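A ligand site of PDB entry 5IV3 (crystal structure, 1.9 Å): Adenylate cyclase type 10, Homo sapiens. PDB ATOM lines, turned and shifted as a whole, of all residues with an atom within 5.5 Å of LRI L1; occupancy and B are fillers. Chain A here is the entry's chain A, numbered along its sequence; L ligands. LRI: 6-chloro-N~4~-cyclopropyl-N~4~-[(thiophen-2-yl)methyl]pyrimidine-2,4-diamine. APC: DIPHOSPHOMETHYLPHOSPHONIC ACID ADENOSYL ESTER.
The backbone carbonyl oxygen of Val 167 is in hydrogen-bond range of a nitrogen (NAA) of LRI L1.
NH2 of Arg 176 is in hydrogen-bond range of O2' of APC L2 (2.8 Å).
The backbone NH (N) of Val 167 is in hydrogen-bond range of a nitrogen (N1) of LRI L1, at 3.2 Å.
A nitrogen (NAA) of LRI L1 sits at hydrogen-bond distance from the backbone carbonyl oxygen (O) of Met 337 (2.9 Å).
N of Met 337 is in hydrogen-bond range of N3 of LRI L1, 3.4 Å away.
Residues that only touch LRI L1: Phe 45, Lys 95, Ala 97, Leu 102, Phe 165, Leu 166, Val 172, Val 175, Arg 176 and Phe 336.
Hydrophobic or aromatic side chains that line LRI L1: Phe 45, Ala 97, Leu 102, Phe 165, Leu 166, Val 167, Val 172, Val 175, Phe 336 and Met 337.
Within 4 Å of LRI L1: Phe 45, Lys 95, Ala 97, Leu 102, Phe 165, Leu 166, Val 167, Val 172, Val 175, Arg 176, Phe 336 and Met 337.
Along chain A the residues within 4 Å of LRI L1 span positions 45 to 337.
The nearest printed residue that does not touch LRI L1 is Leu 94 (4.01 Å).
The backbone carbonyl oxygen (O) of Phe 165 is in hydrogen-bond range of the side-chain amino group (NZ) of Lys 95 (2.7 Å).
The backbone NH of Leu 102 sits at hydrogen-bond distance from the backbone carbonyl oxygen of Lys 95 (3.0 Å).
NZ of Lys 95 lies within hydrogen-bond range of O of Val 335 (2.9 Å).
The backbone carbonyl oxygen of Leu 102 is in hydrogen-bond range of the backbone NH of Leu 94 (2.8 Å).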
ATOM      1  N   PHE A  45     -13.692  31.396  15.327  1.00  0.00           N
ATOM      2  CA  PHE A  45     -13.845  30.201  16.159  1.00  0.00           C
ATOM      3  C   PHE A  45     -13.935  30.632  17.571  1.00  0.00           C
ATOM      4  O   PHE A  45     -12.987  31.289  18.105  1.00  0.00           O
ATOM      5  CB  PHE A  45     -12.697  29.209  15.937  1.00  0.00           C
ATOM      6  CG  PHE A  45     -12.911  27.916  16.640  1.00  0.00           C
ATOM      7  CD1 PHE A  45     -14.132  27.214  16.522  1.00  0.00           C
ATOM      8  CD2 PHE A  45     -11.938  27.416  17.469  1.00  0.00           C
ATOM      9  CE1 PHE A  45     -14.333  26.053  17.219  1.00  0.00           C
ATOM     10  CE2 PHE A  45     -12.136  26.247  18.178  1.00  0.00           C
ATOM     11  CZ  PHE A  45     -13.310  25.555  18.043  1.00  0.00           C
ATOM     12  N   LEU A  94     -21.329  27.772  10.981  1.00  0.00           N
ATOM     13  CA  LEU A  94     -21.095  26.584  10.175  1.00  0.00           C
ATOM     14  C   LEU A  94     -21.415  25.280  10.912  1.00  0.00           C
ATOM     15  O   LEU A  94     -22.082  24.384  10.362  1.00  0.00           O
ATOM     16  CB  LEU A  94     -19.691  26.499   9.644  1.00  0.00           C
ATOM     17  CG  LEU A  94     -19.187  27.616   8.758  1.00  0.00           C
ATOM     18  CD1 LEU A  94     -17.779  27.363   8.196  1.00  0.00           C
ATOM     19  CD2 LEU A  94     -20.160  27.733   7.612  1.00  0.00           C
ATOM     20  N   LYS A  95     -20.858  25.136  12.118  1.00  0.00           N
ATOM     21  CA  LYS A  95     -20.998  23.942  12.887  1.00  0.00           C
ATOM     22  C   LYS A  95     -20.772  24.243  14.372  1.00  0.00           C
ATOM     23  O   LYS A  95     -19.990  25.180  14.708  1.00  0.00           O
ATOM     24  CB  LYS A  95     -20.037  22.898  12.336  1.00  0.00           C
ATOM     25  CG  LYS A  95     -20.331  21.487  12.640  1.00  0.00           C
ATOM     26  CD  LYS A  95     -19.384  20.500  11.896  1.00  0.00           C
ATOM     27  CE  LYS A  95     -19.672  20.269  10.435  1.00  0.00           C
ATOM     28  NZ  LYS A  95     -18.996  18.993   9.937  1.00  0.00           N
ATOM     29  N   PHE A  96     -21.476  23.498  15.240  1.00  0.00           N
ATOM     30  CA  PHE A  96     -21.249  23.478  16.692  1.00  0.00           C
ATOM     31  C   PHE A  96     -20.525  22.195  17.049  1.00  0.00           C
ATOM     32  O   PHE A  96     -20.786  21.137  16.466  1.00  0.00           O
ATOM     33  CB  PHE A  96     -22.529  23.551  17.509  1.00  0.00           C
ATOM     34  CG  PHE A  96     -23.363  24.773  17.308  1.00  0.00           C
ATOM     35  CD1 PHE A  96     -24.182  24.883  16.178  1.00  0.00           C
ATOM     36  CD2 PHE A  96     -23.486  25.745  18.285  1.00  0.00           C
ATOM     37  CE1 PHE A  96     -25.018  25.964  15.983  1.00  0.00           C
ATOM     38  CE2 PHE A  96     -24.275  26.869  18.088  1.00  0.00           C
ATOM     39  CZ  PHE A  96     -25.045  26.991  16.950  1.00  0.00           C
ATOM     40  N   ALA A  97     -19.679  22.277  18.049  1.00  0.00           N
ATOM     41  CA  ALA A  97     -19.035  21.102  18.640  1.00  0.00           C
ATOM     42  C   ALA A  97     -18.929  21.352  20.106  1.00  0.00           C
ATOM     43  O   ALA A  97     -18.160  22.230  20.577  1.00  0.00           O
ATOM     44  CB  ALA A  97     -17.671  20.916  18.070  1.00  0.00           C
ATOM     45  N   ALA A 100     -18.319  24.934  21.572  1.00  0.00           N
ATOM     46  CA  ALA A 100     -17.619  25.765  20.617  1.00  0.00           C
ATOM     47  C   ALA A 100     -18.422  25.864  19.364  1.00  0.00           C
ATOM     48  O   ALA A 100     -19.232  24.961  19.056  1.00  0.00           O
ATOM     49  CB  ALA A 100     -16.299  25.120  20.281  1.00  0.00           C
ATOM     50  N   LEU A 102     -17.948  27.409  15.037  1.00  0.00           N
ATOM     51  CA  LEU A 102     -17.176  28.018  14.004  1.00  0.00           C
ATOM     52  C   LEU A 102     -18.129  28.826  13.125  1.00  0.00           C
ATOM     53  O   LEU A 102     -19.166  28.330  12.673  1.00  0.00           O
ATOM     54  CB  LEU A 102     -16.420  26.951  13.233  1.00  0.00           C
ATOM     55  CG  LEU A 102     -15.573  27.464  12.035  1.00  0.00           C
ATOM     56  CD1 LEU A 102     -14.369  28.248  12.560  1.00  0.00           C
ATOM     57  CD2 LEU A 102     -15.103  26.341  11.111  1.00  0.00           C
ATOM     58  N   PHE A 165     -20.325  18.044   5.591  1.00  0.00           N
ATOM     59  CA  PHE A 165     -19.403  19.049   5.071  1.00  0.00           C
ATOM     60  C   PHE A 165     -18.322  19.491   6.060  1.00  0.00           C
ATOM     61  O   PHE A 165     -18.458  19.335   7.280  1.00  0.00           O
ATOM     62  CB  PHE A 165     -20.123  20.249   4.534  1.00  0.00           C
ATOM     63  CG  PHE A 165     -20.520  21.228   5.591  1.00  0.00           C
ATOM     64  CD1 PHE A 165     -21.609  20.980   6.366  1.00  0.00           C
ATOM     65  CD2 PHE A 165     -19.754  22.355   5.862  1.00  0.00           C
ATOM     66  CE1 PHE A 165     -21.986  21.828   7.372  1.00  0.00           C
ATOM     67  CE2 PHE A 165     -20.155  23.228   6.846  1.00  0.00           C
ATOM     68  CZ  PHE A 165     -21.242  22.917   7.612  1.00  0.00           C
ATOM     69  N   LEU A 166     -17.267  20.099   5.488  1.00  0.00           N
ATOM     70  CA  LEU A 166     -16.154  20.676   6.193  1.00  0.00           C
ATOM     71  C   LEU A 166     -15.675  21.844   5.383  1.00  0.00           C
ATOM     72  O   LEU A 166     -15.786  21.838   4.138  1.00  0.00           O
ATOM     73  CB  LEU A 166     -14.992  19.693   6.192  1.00  0.00           C
ATOM     74  CG  LEU A 166     -15.208  18.424   6.973  1.00  0.00           C
ATOM     75  CD1 LEU A 166     -14.161  17.396   6.645  1.00  0.00           C
ATOM     76  CD2 LEU A 166     -15.162  18.747   8.473  1.00  0.00           C
ATOM     77  N   VAL A 167     -15.114  22.802   6.086  1.00  0.00           N
ATOM     78  CA  VAL A 167     -14.266  23.810   5.440  1.00  0.00           C
ATOM     79  C   VAL A 167     -12.811  23.397   5.670  1.00  0.00           C
ATOM     80  O   VAL A 167     -12.458  22.785   6.667  1.00  0.00           O
ATOM     81  CB  VAL A 167     -14.595  25.249   5.861  1.00  0.00           C
ATOM     82  CG1 VAL A 167     -15.868  25.691   5.218  1.00  0.00           C
ATOM     83  CG2 VAL A 167     -14.635  25.410   7.339  1.00  0.00           C
ATOM     84  N   ILE A 168     -11.989  23.660   4.675  1.00  0.00           N
ATOM     85  CA  ILE A 168     -10.568  23.257   4.692  1.00  0.00           C
ATOM     86  C   ILE A 168      -9.672  24.403   4.169  1.00  0.00           C
ATOM     87  O   ILE A 168     -10.087  25.245   3.340  1.00  0.00           O
ATOM     88  CB  ILE A 168     -10.448  22.039   3.761  1.00  0.00           C
ATOM     89  CG1 ILE A 168     -10.994  20.800   4.489  1.00  0.00           C
ATOM     90  CG2 ILE A 168      -9.029  21.779   3.209  1.00  0.00           C
ATOM     91  CD1 ILE A 168     -11.552  19.836   3.460  1.00  0.00           C
ATOM     92  N   VAL A 172      -8.523  27.938   7.786  1.00  0.00           N
ATOM     93  CA  VAL A 172      -9.168  27.085   8.770  1.00  0.00           C
ATOM     94  C   VAL A 172      -8.186  26.621   9.857  1.00  0.00           C
ATOM     95  O   VAL A 172      -8.476  26.718  11.066  1.00  0.00           O
ATOM     96  CB  VAL A 172      -9.812  25.904   8.046  1.00  0.00           C
ATOM     97  CG1 VAL A 172     -10.493  25.012   9.051  1.00  0.00           C
ATOM     98  CG2 VAL A 172     -10.875  26.365   7.029  1.00  0.00           C
ATOM     99  N   ASP A 173      -7.015  26.154   9.432  1.00  0.00           N
ATOM    100  CA  ASP A 173      -5.932  25.786  10.388  1.00  0.00           C
ATOM    101  C   ASP A 173      -5.565  26.940  11.239  1.00  0.00           C
ATOM    102  O   ASP A 173      -5.512  26.835  12.449  1.00  0.00           O
ATOM    103  CB  ASP A 173      -4.688  25.232   9.685  1.00  0.00           C
ATOM    104  CG  ASP A 173      -4.979  24.004   8.850  1.00  0.00           C
ATOM    105  OD1 ASP A 173      -5.857  23.276   9.253  1.00  0.00           O
ATOM    106  OD2 ASP A 173      -4.326  23.723   7.842  1.00  0.00           O
ATOM    107  N   VAL A 175      -7.390  29.695  12.053  1.00  0.00           N
ATOM    108  CA  VAL A 175      -8.353  30.158  13.061  1.00  0.00           C
ATOM    109  C   VAL A 175      -8.282  29.311  14.326  1.00  0.00           C
ATOM    110  O   VAL A 175      -8.474  29.801  15.482  1.00  0.00           O
ATOM    111  CB  VAL A 175      -9.787  30.267  12.547  1.00  0.00           C
ATOM    112  CG1 VAL A 175     -10.505  28.927  12.434  1.00  0.00           C
ATOM    113  CG2 VAL A 175     -10.600  31.231  13.395  1.00  0.00           C
ATOM    114  N   ARG A 176      -8.107  28.021  14.108  1.00  0.00           N
ATOM    115  CA  ARG A 176      -7.966  27.138  15.260  1.00  0.00           C
ATOM    116  C   ARG A 176      -6.658  27.418  16.062  1.00  0.00           C
ATOM    117  O   ARG A 176      -6.690  27.488  17.310  1.00  0.00           O
ATOM    118  CB  ARG A 176      -8.037  25.697  14.861  1.00  0.00           C
ATOM    119  CG  ARG A 176      -8.548  24.926  16.082  1.00  0.00           C
ATOM    120  CD  ARG A 176      -7.823  23.671  16.372  1.00  0.00           C
ATOM    121  NE  ARG A 176      -6.369  23.767  16.262  1.00  0.00           N
ATOM    122  CZ  ARG A 176      -5.483  23.663  17.282  1.00  0.00           C
ATOM    123  NH1 ARG A 176      -4.186  23.677  16.999  1.00  0.00           N
ATOM    124  NH2 ARG A 176      -5.865  23.541  18.562  1.00  0.00           N
ATOM    125  N   LYS A 334     -20.190  14.043  14.729  1.00  0.00           N
ATOM    126  CA  LYS A 334     -19.626  15.269  14.155  1.00  0.00           C
ATOM    127  C   LYS A 334     -18.331  14.932  13.447  1.00  0.00           C
ATOM    128  O   LYS A 334     -17.668  13.968  13.843  1.00  0.00           O
ATOM    129  CB  LYS A 334     -19.370  16.274  15.290  1.00  0.00           C
ATOM    130  CG  LYS A 334     -19.453  17.770  14.979  1.00  0.00           C
ATOM    131  CD  LYS A 334     -20.810  18.295  14.595  1.00  0.00           C
ATOM    132  CE  LYS A 334     -21.771  18.229  15.773  1.00  0.00           C
ATOM    133  NZ  LYS A 334     -23.044  18.902  15.393  1.00  0.00           N
ATOM    134  N   VAL A 335     -18.010  15.694  12.412  1.00  0.00           N
ATOM    135  CA  VAL A 335     -16.772  15.598  11.654  1.00  0.00           C
ATOM    136  C   VAL A 335     -16.095  16.974  11.694  1.00  0.00           C
ATOM    137  O   VAL A 335     -16.769  17.997  11.575  1.00  0.00           O
ATOM    138  CB  VAL A 335     -17.017  15.140  10.211  1.00  0.00           C
ATOM    139  CG1 VAL A 335     -15.672  14.801   9.590  1.00  0.00           C
ATOM    140  CG2 VAL A 335     -17.995  13.938  10.170  1.00  0.00           C
ATOM    141  N   PHE A 336     -14.774  16.960  11.874  1.00  0.00           N
ATOM    142  CA  PHE A 336     -13.890  18.140  12.052  1.00  0.00           C
ATOM    143  C   PHE A 336     -12.654  17.970  11.165  1.00  0.00           C
ATOM    144  O   PHE A 336     -12.240  16.840  10.903  1.00  0.00           O
ATOM    145  CB  PHE A 336     -13.270  18.174  13.432  1.00  0.00           C
ATOM    146  CG  PHE A 336     -14.207  17.980  14.508  1.00  0.00           C
ATOM    147  CD1 PHE A 336     -14.985  19.005  14.890  1.00  0.00           C
ATOM    148  CD2 PHE A 336     -14.342  16.749  15.131  1.00  0.00           C
ATOM    149  CE1 PHE A 336     -15.907  18.824  15.922  1.00  0.00           C
ATOM    150  CE2 PHE A 336     -15.212  16.574  16.176  1.00  0.00           C
ATOM    151  CZ  PHE A 336     -16.009  17.602  16.579  1.00  0.00           C
ATOM    152  N   MET A 337     -12.042  19.081  10.781  1.00  0.00           N
ATOM    153  CA  MET A 337     -10.692  19.036  10.146  1.00  0.00           C
ATOM    154  C   MET A 337      -9.834  20.266  10.388  1.00  0.00           C
ATOM    155  O   MET A 337     -10.260  21.370  10.176  1.00  0.00           O
ATOM    156  CB  MET A 337     -10.743  18.813   8.638  1.00  0.00           C
ATOM    157  CG  MET A 337      -9.340  18.562   8.035  1.00  0.00           C
ATOM    158  SD  MET A 337      -9.401  17.830   6.419  1.00  0.00           S
ATOM    159  CE  MET A 337      -7.641  17.555   6.284  1.00  0.00           C
ATOM    160  N   PHE A 338      -8.610  20.035  10.864  1.00  0.00           N
ATOM    161  CA  PHE A 338      -7.603  21.139  11.033  1.00  0.00           C
ATOM    162  C   PHE A 338      -6.238  20.457  11.159  1.00  0.00           C
ATOM    163  O   PHE A 338      -6.206  19.250  11.401  1.00  0.00           O
ATOM    164  CB  PHE A 338      -7.911  22.034  12.218  1.00  0.00           C
ATOM    165  CG  PHE A 338      -8.166  21.277  13.480  1.00  0.00           C
ATOM    166  CD1 PHE A 338      -7.106  20.929  14.333  1.00  0.00           C
ATOM    167  CD2 PHE A 338      -9.469  20.931  13.846  1.00  0.00           C
ATOM    168  CE1 PHE A 338      -7.361  20.220  15.525  1.00  0.00           C
ATOM    169  CE2 PHE A 338      -9.714  20.234  15.045  1.00  0.00           C
ATOM    170  CZ  PHE A 338      -8.656  19.860  15.862  1.00  0.00           C
HETATM  171  CAL LRI L   1     -12.444  24.569  14.556  1.00  0.00           C
HETATM  172  CAM LRI L   1     -11.647  25.553  14.073  1.00  0.00           C
HETATM  173  CAN LRI L   1     -11.206  25.461  12.776  1.00  0.00           C
HETATM  174  SAO LRI L   1     -11.726  23.974  12.228  1.00  0.00           S
HETATM  175  CAK LRI L   1     -12.552  23.564  13.650  1.00  0.00           C
HETATM  176  CAJ LRI L   1     -13.338  22.247  13.744  1.00  0.00           C
HETATM  177  NAI LRI L   1     -14.693  22.392  13.236  1.00  0.00           N
HETATM  178  CAP LRI L   1     -15.592  23.155  14.129  1.00  0.00           C
HETATM  179  CAQ LRI L   1     -16.958  22.527  14.534  1.00  0.00           C
HETATM  180  CAR LRI L   1     -15.754  22.562  15.474  1.00  0.00           C
HETATM  181  C4  LRI L   1     -14.889  22.328  11.929  1.00  0.00           C
HETATM  182  N3  LRI L   1     -13.886  21.966  11.133  1.00  0.00           N
HETATM  183  C5  LRI L   1     -16.093  22.702  11.332  1.00  0.00           C
HETATM  184  C6  LRI L   1     -16.138  22.686   9.959  1.00  0.00           C
HETATM  185 CL6  LRI L   1     -17.536  23.165   9.107  1.00  0.00          CL
HETATM  186  N1  LRI L   1     -15.077  22.406   9.255  1.00  0.00           N
HETATM  187  C2  LRI L   1     -13.955  22.025   9.841  1.00  0.00           C
HETATM  188  NAA LRI L   1     -12.897  21.707   9.103  1.00  0.00           N
HETATM  189  PG  APC L   2     -13.884  22.633  27.832  1.00  0.00           P
HETATM  190  O1G APC L   2     -13.582  21.241  27.457  1.00  0.00           O
HETATM  191  O2G APC L   2     -14.965  23.123  26.935  1.00  0.00           O
HETATM  192  O3G APC L   2     -14.782  23.002  29.025  1.00  0.00           O
HETATM  193  PB  APC L   2     -11.634  23.595  26.300  1.00  0.00           P
HETATM  194  O1B APC L   2     -11.960  23.915  24.802  1.00  0.00           O
HETATM  195  O2B APC L   2     -10.683  24.557  26.890  1.00  0.00           O
HETATM  196  O3B APC L   2     -12.741  23.696  27.493  1.00  0.00           O
HETATM  197  PA  APC L   2      -9.223  21.924  25.754  1.00  0.00           P
HETATM  198  O1A APC L   2      -8.643  20.422  25.737  1.00  0.00           O
HETATM  199  O2A APC L   2      -8.376  22.740  26.698  1.00  0.00           O
HETATM  200  C3A APC L   2     -10.983  21.912  26.218  1.00  0.00           C
HETATM  201  O5' APC L   2      -9.123  22.525  24.302  1.00  0.00           O
HETATM  202  C5' APC L   2      -7.727  22.758  24.008  1.00  0.00           C
HETATM  203  C4' APC L   2      -7.585  23.131  22.574  1.00  0.00           C
HETATM  204  O4' APC L   2      -7.974  22.087  21.664  1.00  0.00           O
HETATM  205  C3' APC L   2      -8.566  24.294  22.379  1.00  0.00           C
HETATM  206  O3' APC L   2      -8.040  25.491  22.959  1.00  0.00           O
HETATM  207  C2' APC L   2      -8.844  24.233  20.896  1.00  0.00           C
HETATM  208  O2' APC L   2      -7.834  24.849  20.101  1.00  0.00           O
HETATM  209  C1' APC L   2      -8.847  22.723  20.707  1.00  0.00           C
HETATM  210  N9  APC L   2     -10.301  22.327  20.792  1.00  0.00           N
HETATM  211  C8  APC L   2     -11.169  22.079  21.829  1.00  0.00           C
HETATM  212  N7  APC L   2     -12.390  21.767  21.331  1.00  0.00           N
HETATM  213  C5  APC L   2     -12.299  21.852  19.956  1.00  0.00           C
HETATM  214  C6  APC L   2     -13.126  21.669  18.728  1.00  0.00           C
HETATM  215  N6  APC L   2     -14.385  21.331  18.781  1.00  0.00           N
HETATM  216  N1  APC L   2     -12.618  21.818  17.501  1.00  0.00           N
HETATM  217  C2  APC L   2     -11.325  22.142  17.304  1.00  0.00           C
HETATM  218  N3  APC L   2     -10.501  22.331  18.337  1.00  0.00           N
HETATM  219  C4  APC L   2     -10.932  22.198  19.624  1.00  0.00           C
